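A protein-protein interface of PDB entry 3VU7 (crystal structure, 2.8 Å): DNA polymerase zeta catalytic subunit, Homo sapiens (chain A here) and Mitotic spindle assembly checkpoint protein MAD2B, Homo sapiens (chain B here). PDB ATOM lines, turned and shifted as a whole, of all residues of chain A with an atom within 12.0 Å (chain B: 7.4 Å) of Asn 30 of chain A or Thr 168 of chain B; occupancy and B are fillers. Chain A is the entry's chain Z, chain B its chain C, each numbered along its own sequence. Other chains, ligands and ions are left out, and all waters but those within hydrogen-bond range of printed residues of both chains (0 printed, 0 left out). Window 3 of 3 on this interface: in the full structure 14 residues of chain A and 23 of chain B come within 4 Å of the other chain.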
ATOM      1  N   ARG A  27       4.876 -26.628  40.912  1.00  0.00           N
ATOM      2  CA  ARG A  27       3.396 -26.749  41.002  1.00  0.00           C
ATOM      3  C   ARG A  27       2.910 -27.546  39.807  1.00  0.00           C
ATOM      4  O   ARG A  27       2.651 -26.989  38.740  1.00  0.00           O
ATOM      5  CB  ARG A  27       2.741 -25.351  41.018  1.00  0.00           C
ATOM      6  CG  ARG A  27       1.558 -25.221  42.051  1.00  0.00           C
ATOM      7  CD  ARG A  27       0.241 -25.398  41.278  1.00  0.00           C
ATOM      8  NE  ARG A  27      -0.968 -25.491  42.127  1.00  0.00           N
ATOM      9  CZ  ARG A  27      -2.165 -25.850  41.644  1.00  0.00           C
ATOM     10  NH1 ARG A  27      -2.273 -26.158  40.340  1.00  0.00           N
ATOM     11  NH2 ARG A  27      -3.242 -25.904  42.428  1.00  0.00           N
ATOM     12  N   THR A  28       2.803 -28.860  39.994  1.00  0.00           N
ATOM     13  CA  THR A  28       2.325 -29.767  38.954  1.00  0.00           C
ATOM     14  C   THR A  28       3.096 -29.663  37.627  1.00  0.00           C
ATOM     15  O   THR A  28       4.041 -28.880  37.481  1.00  0.00           O
ATOM     16  CB  THR A  28       0.791 -29.650  38.742  1.00  0.00           C
ATOM     17  OG1 THR A  28       0.384 -28.265  38.829  1.00  0.00           O
ATOM     18  CG2 THR A  28       0.049 -30.449  39.799  1.00  0.00           C
ATOM     19  N   ALA A  29       2.687 -30.482  36.665  1.00  0.00           N
ATOM     20  CA  ALA A  29       3.429 -30.634  35.432  1.00  0.00           C
ATOM     21  C   ALA A  29       2.531 -31.026  34.275  1.00  0.00           C
ATOM     22  O   ALA A  29       2.683 -32.117  33.690  1.00  0.00           O
ATOM     23  CB  ALA A  29       4.522 -31.668  35.624  1.00  0.00           C
ATOM     24  N   ASN A  30       1.592 -30.117  33.960  1.00  0.00           N
ATOM     25  CA  ASN A  30       0.739 -30.265  32.805  1.00  0.00           C
ATOM     26  C   ASN A  30       1.080 -29.148  31.847  1.00  0.00           C
ATOM     27  O   ASN A  30       0.323 -28.859  30.928  1.00  0.00           O
ATOM     28  CB  ASN A  30      -0.725 -30.147  33.218  1.00  0.00           C
ATOM     29  CG  ASN A  30      -1.066 -28.768  33.721  1.00  0.00           C
ATOM     30  OD1 ASN A  30      -0.533 -28.319  34.740  1.00  0.00           O
ATOM     31  ND2 ASN A  30      -1.945 -28.082  32.996  1.00  0.00           N
ATOM     32  N   ILE A  31       2.220 -28.506  32.098  1.00  0.00           N
ATOM     33  CA  ILE A  31       2.756 -27.463  31.224  1.00  0.00           C
ATOM     34  C   ILE A  31       3.937 -27.938  30.363  1.00  0.00           C
ATOM     35  O   ILE A  31       4.981 -28.331  30.892  1.00  0.00           O
ATOM     36  CB  ILE A  31       3.269 -26.262  32.032  1.00  0.00           C
ATOM     37  CG1 ILE A  31       2.432 -26.015  33.276  1.00  0.00           C
ATOM     38  CG2 ILE A  31       3.414 -25.029  31.150  1.00  0.00           C
ATOM     39  CD1 ILE A  31       3.072 -26.645  34.501  1.00  0.00           C
ATOM     40  N   LEU A  32       3.789 -27.862  29.043  1.00  0.00           N
ATOM     41  CA  LEU A  32       4.859 -28.275  28.141  1.00  0.00           C
ATOM     42  C   LEU A  32       5.552 -27.134  27.466  1.00  0.00           C
ATOM     43  O   LEU A  32       4.963 -26.121  27.163  1.00  0.00           O
ATOM     44  CB  LEU A  32       4.326 -29.217  27.080  1.00  0.00           C
ATOM     45  CG  LEU A  32       3.748 -30.500  27.642  1.00  0.00           C
ATOM     46  CD1 LEU A  32       3.074 -31.314  26.560  1.00  0.00           C
ATOM     47  CD2 LEU A  32       4.858 -31.308  28.256  1.00  0.00           C
ATOM     48  N   LYS A  33       6.812 -27.351  27.172  1.00  0.00           N
ATOM     49  CA  LYS A  33       7.705 -26.308  26.715  1.00  0.00           C
ATOM     50  C   LYS A  33       8.602 -26.991  25.696  1.00  0.00           C
ATOM     51  O   LYS A  33       8.891 -28.169  25.869  1.00  0.00           O
ATOM     52  CB  LYS A  33       8.515 -25.838  27.930  1.00  0.00           C
ATOM     53  CG  LYS A  33       9.544 -24.756  27.748  1.00  0.00           C
ATOM     54  CD  LYS A  33      10.566 -24.911  28.873  1.00  0.00           C
ATOM     55  CE  LYS A  33      11.742 -23.915  28.865  1.00  0.00           C
ATOM     56  NZ  LYS A  33      12.534 -23.726  27.596  1.00  0.00           N
ATOM     57  N   PRO A  34       9.020 -26.277  24.620  1.00  0.00           N
ATOM     58  CA  PRO A  34      10.037 -26.799  23.746  1.00  0.00           C
ATOM     59  C   PRO A  34      11.350 -26.694  24.455  1.00  0.00           C
ATOM     60  O   PRO A  34      11.513 -25.821  25.298  1.00  0.00           O
ATOM     61  CB  PRO A  34      10.019 -25.823  22.579  1.00  0.00           C
ATOM     62  CG  PRO A  34       8.666 -25.263  22.581  1.00  0.00           C
ATOM     63  CD  PRO A  34       8.450 -25.054  24.045  1.00  0.00           C
ATOM     64  N   LEU B  90      -2.521 -32.218  19.680  1.00  0.00           N
ATOM     65  CA  LEU B  90      -3.110 -32.115  21.007  1.00  0.00           C
ATOM     66  C   LEU B  90      -4.385 -31.269  20.965  1.00  0.00           C
ATOM     67  O   LEU B  90      -5.288 -31.431  21.798  1.00  0.00           O
ATOM     68  CB  LEU B  90      -2.115 -31.505  21.975  1.00  0.00           C
ATOM     69  CG  LEU B  90      -1.189 -32.481  22.703  1.00  0.00           C
ATOM     70  CD1 LEU B  90      -0.249 -33.231  21.751  1.00  0.00           C
ATOM     71  CD2 LEU B  90      -0.387 -31.750  23.771  1.00  0.00           C
ATOM     72  N   ASN B  94      -8.300 -32.279  21.626  1.00  0.00           N
ATOM     73  CA  ASN B  94      -8.719 -31.329  22.636  1.00  0.00           C
ATOM     74  C   ASN B  94      -8.093 -31.497  24.043  1.00  0.00           C
ATOM     75  O   ASN B  94      -8.799 -31.437  25.053  1.00  0.00           O
ATOM     76  CB  ASN B  94     -10.246 -31.281  22.705  1.00  0.00           C
ATOM     77  CG  ASN B  94     -10.758 -30.115  23.534  1.00  0.00           C
ATOM     78  OD1 ASN B  94     -10.038 -29.168  23.850  1.00  0.00           O
ATOM     79  ND2 ASN B  94     -11.999 -30.188  23.896  1.00  0.00           N
ATOM     80  N   ASP B  95      -6.773 -31.658  24.127  1.00  0.00           N
ATOM     81  CA  ASP B  95      -6.133 -31.826  25.453  1.00  0.00           C
ATOM     82  C   ASP B  95      -5.457 -30.586  26.011  1.00  0.00           C
ATOM     83  O   ASP B  95      -5.102 -30.537  27.186  1.00  0.00           O
ATOM     84  CB  ASP B  95      -5.191 -33.020  25.443  1.00  0.00           C
ATOM     85  CG  ASP B  95      -5.952 -34.337  25.280  1.00  0.00           C
ATOM     86  OD1 ASP B  95      -6.596 -34.756  26.274  1.00  0.00           O
ATOM     87  OD2 ASP B  95      -5.939 -34.925  24.160  1.00  0.00           O
ATOM     88  N   VAL B  96      -5.296 -29.596  25.139  1.00  0.00           N
ATOM     89  CA  VAL B  96      -4.709 -28.316  25.452  1.00  0.00           C
ATOM     90  C   VAL B  96      -5.779 -27.443  26.014  1.00  0.00           C
ATOM     91  O   VAL B  96      -6.875 -27.324  25.451  1.00  0.00           O
ATOM     92  CB  VAL B  96      -4.191 -27.633  24.187  1.00  0.00           C
ATOM     93  CG1 VAL B  96      -3.610 -26.268  24.519  1.00  0.00           C
ATOM     94  CG2 VAL B  96      -3.157 -28.522  23.506  1.00  0.00           C
ATOM     95  N   GLU B  97      -5.438 -26.842  27.140  1.00  0.00           N
ATOM     96  CA  GLU B  97      -6.330 -25.978  27.879  1.00  0.00           C
ATOM     97  C   GLU B  97      -6.015 -24.529  27.520  1.00  0.00           C
ATOM     98  O   GLU B  97      -6.940 -23.780  27.217  1.00  0.00           O
ATOM     99  CB  GLU B  97      -6.125 -26.194  29.369  1.00  0.00           C
ATOM    100  CG  GLU B  97      -6.750 -25.106  30.222  1.00  0.00           C
ATOM    101  CD  GLU B  97      -6.051 -24.919  31.556  1.00  0.00           C
ATOM    102  OE1 GLU B  97      -6.462 -23.990  32.313  1.00  0.00           O
ATOM    103  OE2 GLU B  97      -5.088 -25.690  31.829  1.00  0.00           O
ATOM    104  N   LYS B  98      -4.729 -24.137  27.587  1.00  0.00           N
ATOM    105  CA  LYS B  98      -4.284 -22.818  27.089  1.00  0.00           C
ATOM    106  C   LYS B  98      -2.952 -22.908  26.377  1.00  0.00           C
ATOM    107  O   LYS B  98      -2.121 -23.781  26.703  1.00  0.00           O
ATOM    108  CB  LYS B  98      -4.273 -21.683  28.151  1.00  0.00           C
ATOM    109  CG  LYS B  98      -3.710 -22.042  29.516  1.00  0.00           C
ATOM    110  CD  LYS B  98      -3.471 -20.804  30.358  1.00  0.00           C
ATOM    111  CE  LYS B  98      -3.815 -21.001  31.817  1.00  0.00           C
ATOM    112  NZ  LYS B  98      -5.255 -20.670  31.970  1.00  0.00           N
ATOM    113  N   LEU B 165       4.379 -21.890  25.753  1.00  0.00           N
ATOM    114  CA  LEU B 165       4.015 -22.856  26.790  1.00  0.00           C
ATOM    115  C   LEU B 165       2.653 -23.400  26.420  1.00  0.00           C
ATOM    116  O   LEU B 165       1.762 -22.650  25.990  1.00  0.00           O
ATOM    117  CB  LEU B 165       3.921 -22.184  28.162  1.00  0.00           C
ATOM    118  CG  LEU B 165       5.184 -21.591  28.800  1.00  0.00           C
ATOM    119  CD1 LEU B 165       4.906 -21.141  30.226  1.00  0.00           C
ATOM    120  CD2 LEU B 165       6.218 -22.677  28.801  1.00  0.00           C
ATOM    121  N   VAL B 166       2.495 -24.708  26.554  1.00  0.00           N
ATOM    122  CA  VAL B 166       1.225 -25.350  26.270  1.00  0.00           C
ATOM    123  C   VAL B 166       0.702 -25.951  27.568  1.00  0.00           C
ATOM    124  O   VAL B 166       1.267 -26.931  28.066  1.00  0.00           O
ATOM    125  CB  VAL B 166       1.427 -26.499  25.280  1.00  0.00           C
ATOM    126  CG1 VAL B 166       0.091 -27.129  24.935  1.00  0.00           C
ATOM    127  CG2 VAL B 166       2.117 -25.991  24.045  1.00  0.00           C
ATOM    128  N   HIS B 167      -0.341 -25.365  28.142  1.00  0.00           N
ATOM    129  CA  HIS B 167      -0.948 -25.952  29.340  1.00  0.00           C
ATOM    130  C   HIS B 167      -1.941 -27.020  28.962  1.00  0.00           C
ATOM    131  O   HIS B 167      -3.030 -26.716  28.423  1.00  0.00           O
ATOM    132  CB  HIS B 167      -1.689 -24.889  30.107  1.00  0.00           C
ATOM    133  CG  HIS B 167      -0.803 -23.899  30.804  1.00  0.00           C
ATOM    134  ND1 HIS B 167      -0.028 -23.008  30.127  1.00  0.00           N
ATOM    135  CD2 HIS B 167      -0.625 -23.641  32.157  1.00  0.00           C
ATOM    136  CE1 HIS B 167       0.626 -22.224  31.009  1.00  0.00           C
ATOM    137  NE2 HIS B 167       0.269 -22.623  32.256  1.00  0.00           N
ATOM    138  N   THR B 168      -1.606 -28.283  29.225  1.00  0.00           N
ATOM    139  CA  THR B 168      -2.618 -29.370  29.011  1.00  0.00           C
ATOM    140  C   THR B 168      -3.762 -29.406  30.049  1.00  0.00           C
ATOM    141  O   THR B 168      -3.613 -28.930  31.193  1.00  0.00           O
ATOM    142  CB  THR B 168      -1.964 -30.763  28.936  1.00  0.00           C
ATOM    143  OG1 THR B 168      -1.123 -30.995  30.091  1.00  0.00           O
ATOM    144  CG2 THR B 168      -1.149 -30.866  27.655  1.00  0.00           C
ATOM    145  N   ARG B 169      -4.890 -29.987  29.664  1.00  0.00           N
ATOM    146  CA  ARG B 169      -6.024 -30.101  30.575  1.00  0.00           C
ATOM    147  C   ARG B 169      -5.678 -31.084  31.667  1.00  0.00           C
ATOM    148  O   ARG B 169      -5.980 -30.895  32.839  1.00  0.00           O
ATOM    149  CB  ARG B 169      -7.252 -30.623  29.838  1.00  0.00           C
ATOM    150  CG  ARG B 169      -7.803 -29.719  28.746  1.00  0.00           C
ATOM    151  CD  ARG B 169      -9.212 -30.092  28.332  1.00  0.00           C
ATOM    152  NE  ARG B 169      -9.612 -29.311  27.168  1.00  0.00           N
ATOM    153  CZ  ARG B 169      -9.894 -27.989  27.187  1.00  0.00           C
ATOM    154  NH1 ARG B 169      -9.808 -27.284  28.330  1.00  0.00           N
ATOM    155  NH2 ARG B 169     -10.256 -27.349  26.055  1.00  0.00           N
ATOM    156  N   GLU B 170      -5.044 -32.164  31.256  1.00  0.00           N
ATOM    157  CA  GLU B 170      -4.806 -33.284  32.139  1.00  0.00           C
ATOM    158  C   GLU B 170      -3.307 -33.445  32.220  1.00  0.00           C
ATOM    159  O   GLU B 170      -2.587 -33.163  31.248  1.00  0.00           O
ATOM    160  CB  GLU B 170      -5.483 -34.547  31.563  1.00  0.00           C
ATOM    161  CG  GLU B 170      -5.435 -34.686  30.011  1.00  0.00           C
ATOM    162  CD  GLU B 170      -6.077 -35.985  29.448  1.00  0.00           C
ATOM    163  OE1 GLU B 170      -5.723 -36.424  28.319  1.00  0.00           O
ATOM    164  OE2 GLU B 170      -6.934 -36.593  30.128  1.00  0.00           O
ATOM    165  N   ALA B 171      -2.813 -33.857  33.373  1.00  0.00           N
ATOM    166  CA  ALA B 171      -1.406 -34.203  33.446  1.00  0.00           C
ATOM    167  C   ALA B 171      -1.255 -35.627  32.931  1.00  0.00           C
ATOM    168  O   ALA B 171      -1.483 -36.590  33.647  1.00  0.00           O
ATOM    169  CB  ALA B 171      -0.873 -34.059  34.862  1.00  0.00           C
ATOM    170  N   ALA B 172      -0.890 -35.782  31.675  1.00  0.00           N
ATOM    171  CA  ALA B 172      -0.964 -37.109  31.090  1.00  0.00           C
ATOM    172  C   ALA B 172       0.211 -37.481  30.211  1.00  0.00           C
ATOM    173  O   ALA B 172       0.577 -36.794  29.281  1.00  0.00           O
ATOM    174  CB  ALA B 172      -2.279 -37.282  30.347  1.00  0.00           C
ATOM    175  N   ASN B 175      -0.182 -37.092  26.548  1.00  0.00           N
ATOM    176  CA  ASN B 175       0.246 -35.755  26.111  1.00  0.00           C
ATOM    177  C   ASN B 175       1.731 -35.594  25.682  1.00  0.00           C
ATOM    178  O   ASN B 175       2.033 -34.977  24.665  1.00  0.00           O
ATOM    179  CB  ASN B 175      -0.039 -34.745  27.218  1.00  0.00           C
ATOM    180  CG  ASN B 175      -1.513 -34.528  27.449  1.00  0.00           C
ATOM    181  OD1 ASN B 175      -2.335 -34.726  26.554  1.00  0.00           O
ATOM    182  ND2 ASN B 175      -1.856 -34.086  28.652  1.00  0.00           N
ATOM    183  N   MET B 176       2.654 -36.131  26.462  1.00  0.00           N
ATOM    184  CA  MET B 176       4.058 -36.040  26.112  1.00  0.00           C
ATOM    185  C   MET B 176       4.314 -36.812  24.826  1.00  0.00           C
ATOM    186  O   MET B 176       5.068 -36.375  23.970  1.00  0.00           O
ATOM    187  CB  MET B 176       4.908 -36.595  27.238  1.00  0.00           C
ATOM    188  CG  MET B 176       6.379 -36.309  27.065  1.00  0.00           C
ATOM    189  SD  MET B 176       6.965 -35.123  28.279  1.00  0.00           S
ATOM    190  CE  MET B 176       8.675 -34.876  27.783  1.00  0.00           C
ATOM    191  N   ILE B 179       2.913 -35.022  21.665  1.00  0.00           N
ATOM    192  CA  ILE B 179       3.644 -33.795  21.378  1.00  0.00           C
ATOM    193  C   ILE B 179       5.049 -34.068  20.804  1.00  0.00           C
ATOM    194  O   ILE B 179       5.515 -33.286  19.966  1.00  0.00           O
ATOM    195  CB  ILE B 179       3.644 -32.764  22.546  1.00  0.00           C
ATOM    196  CG1 ILE B 179       3.793 -31.342  22.002  1.00  0.00           C
ATOM    197  CG2 ILE B 179       4.711 -33.072  23.587  1.00  0.00           C
ATOM    198  CD1 ILE B 179       3.599 -30.199  22.998  1.00  0.00           C
ATOM    199  N   LEU B 189       9.127 -30.757  30.356  1.00  0.00           N
ATOM    200  CA  LEU B 189       8.196 -30.142  31.290  1.00  0.00           C
ATOM    201  C   LEU B 189       8.803 -28.815  31.693  1.00  0.00           C
ATOM    202  O   LEU B 189      10.025 -28.727  31.800  1.00  0.00           O
ATOM    203  CB  LEU B 189       7.980 -31.031  32.506  1.00  0.00           C
ATOM    204  CG  LEU B 189       7.237 -32.338  32.231  1.00  0.00           C
ATOM    205  CD1 LEU B 189       7.749 -33.424  33.154  1.00  0.00           C
ATOM    206  CD2 LEU B 189       5.744 -32.177  32.403  1.00  0.00           C
ATOM    207  N   ALA B 190       7.958 -27.793  31.874  1.00  0.00           N
ATOM    208  CA  ALA B 190       8.366 -26.445  32.303  1.00  0.00           C
ATOM    209  C   ALA B 190       8.869 -26.432  33.744  1.00  0.00           C
ATOM    210  O   ALA B 190       8.425 -27.250  34.544  1.00  0.00           O
ATOM    211  CB  ALA B 190       7.176 -25.514  32.187  1.00  0.00           C
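Ala 29 of chain A touches Leu 189 of chain B.
Asn 30 of chain A touches Val 166 of chain B (O to O, 3.6 Å).
His 167 of chain B touches Asn 30 of chain A (C to O, 3.5 Å).
O of Val 166 of chain B touches CA of Ile 31 of chain A (3.5 Å).
CE1 of His 167 of chain B touches CG2 of Ile 31 of chain A (3.96 Å).
Ile 31 of chain A touches Leu 189 of chain B (O to CA, 3.7 Å).
Leu 165 of chain B touches Leu 32 of chain A (CA to O, 3.4 Å).
Leu 32 of chain A touches Ile 179 of chain B.
O of Ile 31 of chain A lies within hydrogen-bond range of N of Ala 190 of chain B.
O of Thr 168 of chain B sits at hydrogen-bond distance from ND2 of Asn 30 of chain A (2.6 Å).
The backbone carbonyl oxygen (O) of Val 166 of chain B sits at hydrogen-bond distance from the backbone NH (N) of Leu 32 of chain A (2.9 Å).
The backbone NH (N) of His 167 of chain B sits at hydrogen-bond distance from the backbone carbonyl oxygen (O) of Lys 98 of chain B.
N of Glu 97 of chain B lies within hydrogen-bond range of O of His 167 of chain B (2.7 Å).
The side-chain amide nitrogen of Asn 175 of chain B sits close to the side-chain hydroxyl of Thr 168 of chain B.
OG1 of Thr 168 of chain B lies within hydrogen-bond range of O of Glu 170 of chain B (2.9 Å).
Of chain B, only Val 166, His 167 and Thr 168 come within 4 Å of Asn 30 of chain A.
Of chain A, only Asn 30 (2.6 Å) comes within 4 Å of Thr 168 of chain B.
No residue of chain A comes within 4 Å of Glu 97 of chain B.
Val 166 of chain B touches just these residues of chain A: Asn 30 (3.6 Å), Ile 31 (3.5 Å) and Leu 32 (2.9 Å).
Of chain A, only Asn 30 (3.5 Å) and Ile 31 (3.96 Å) come within 4 Å of His 167 of chain B.
No residue of chain A comes within 4 Å of Arg 169 of chain B.
Glu 170 of chain B touches none of the printed residues of chain A.
No residue of chain A comes within 4 Å of Ala 171 of chain B.
No residue of chain A comes within 4 Å of Asn 175 of chain B.
Of the printed residues of chain B, Leu 32 of chain A touches Leu 165, Val 166 and Ile 179.
Printed residues of chain A within 4 Å of Leu 189 of chain B: Ala 29 (3.3 Å) and Ile 31 (3.7 Å).
Pro 34 of chain A touches none of the printed residues of chain B.
Lys 98 of chain B touches none of the printed residues of chain A.
The nearest residue of chain B that does not touch Asn 30 of chain A is Glu 170 of chain B (4.1 Å).
Printed residues of chain B that touch a printed residue of chain A: Leu 165, Val 166, His 167, Thr 168, Ile 179, Leu 189 and Ala 190.
Along chain B the printed residues that touch a printed residue of chain A span positions 165 to 190.
Among the printed residues, 11 pairs touch across the chains.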
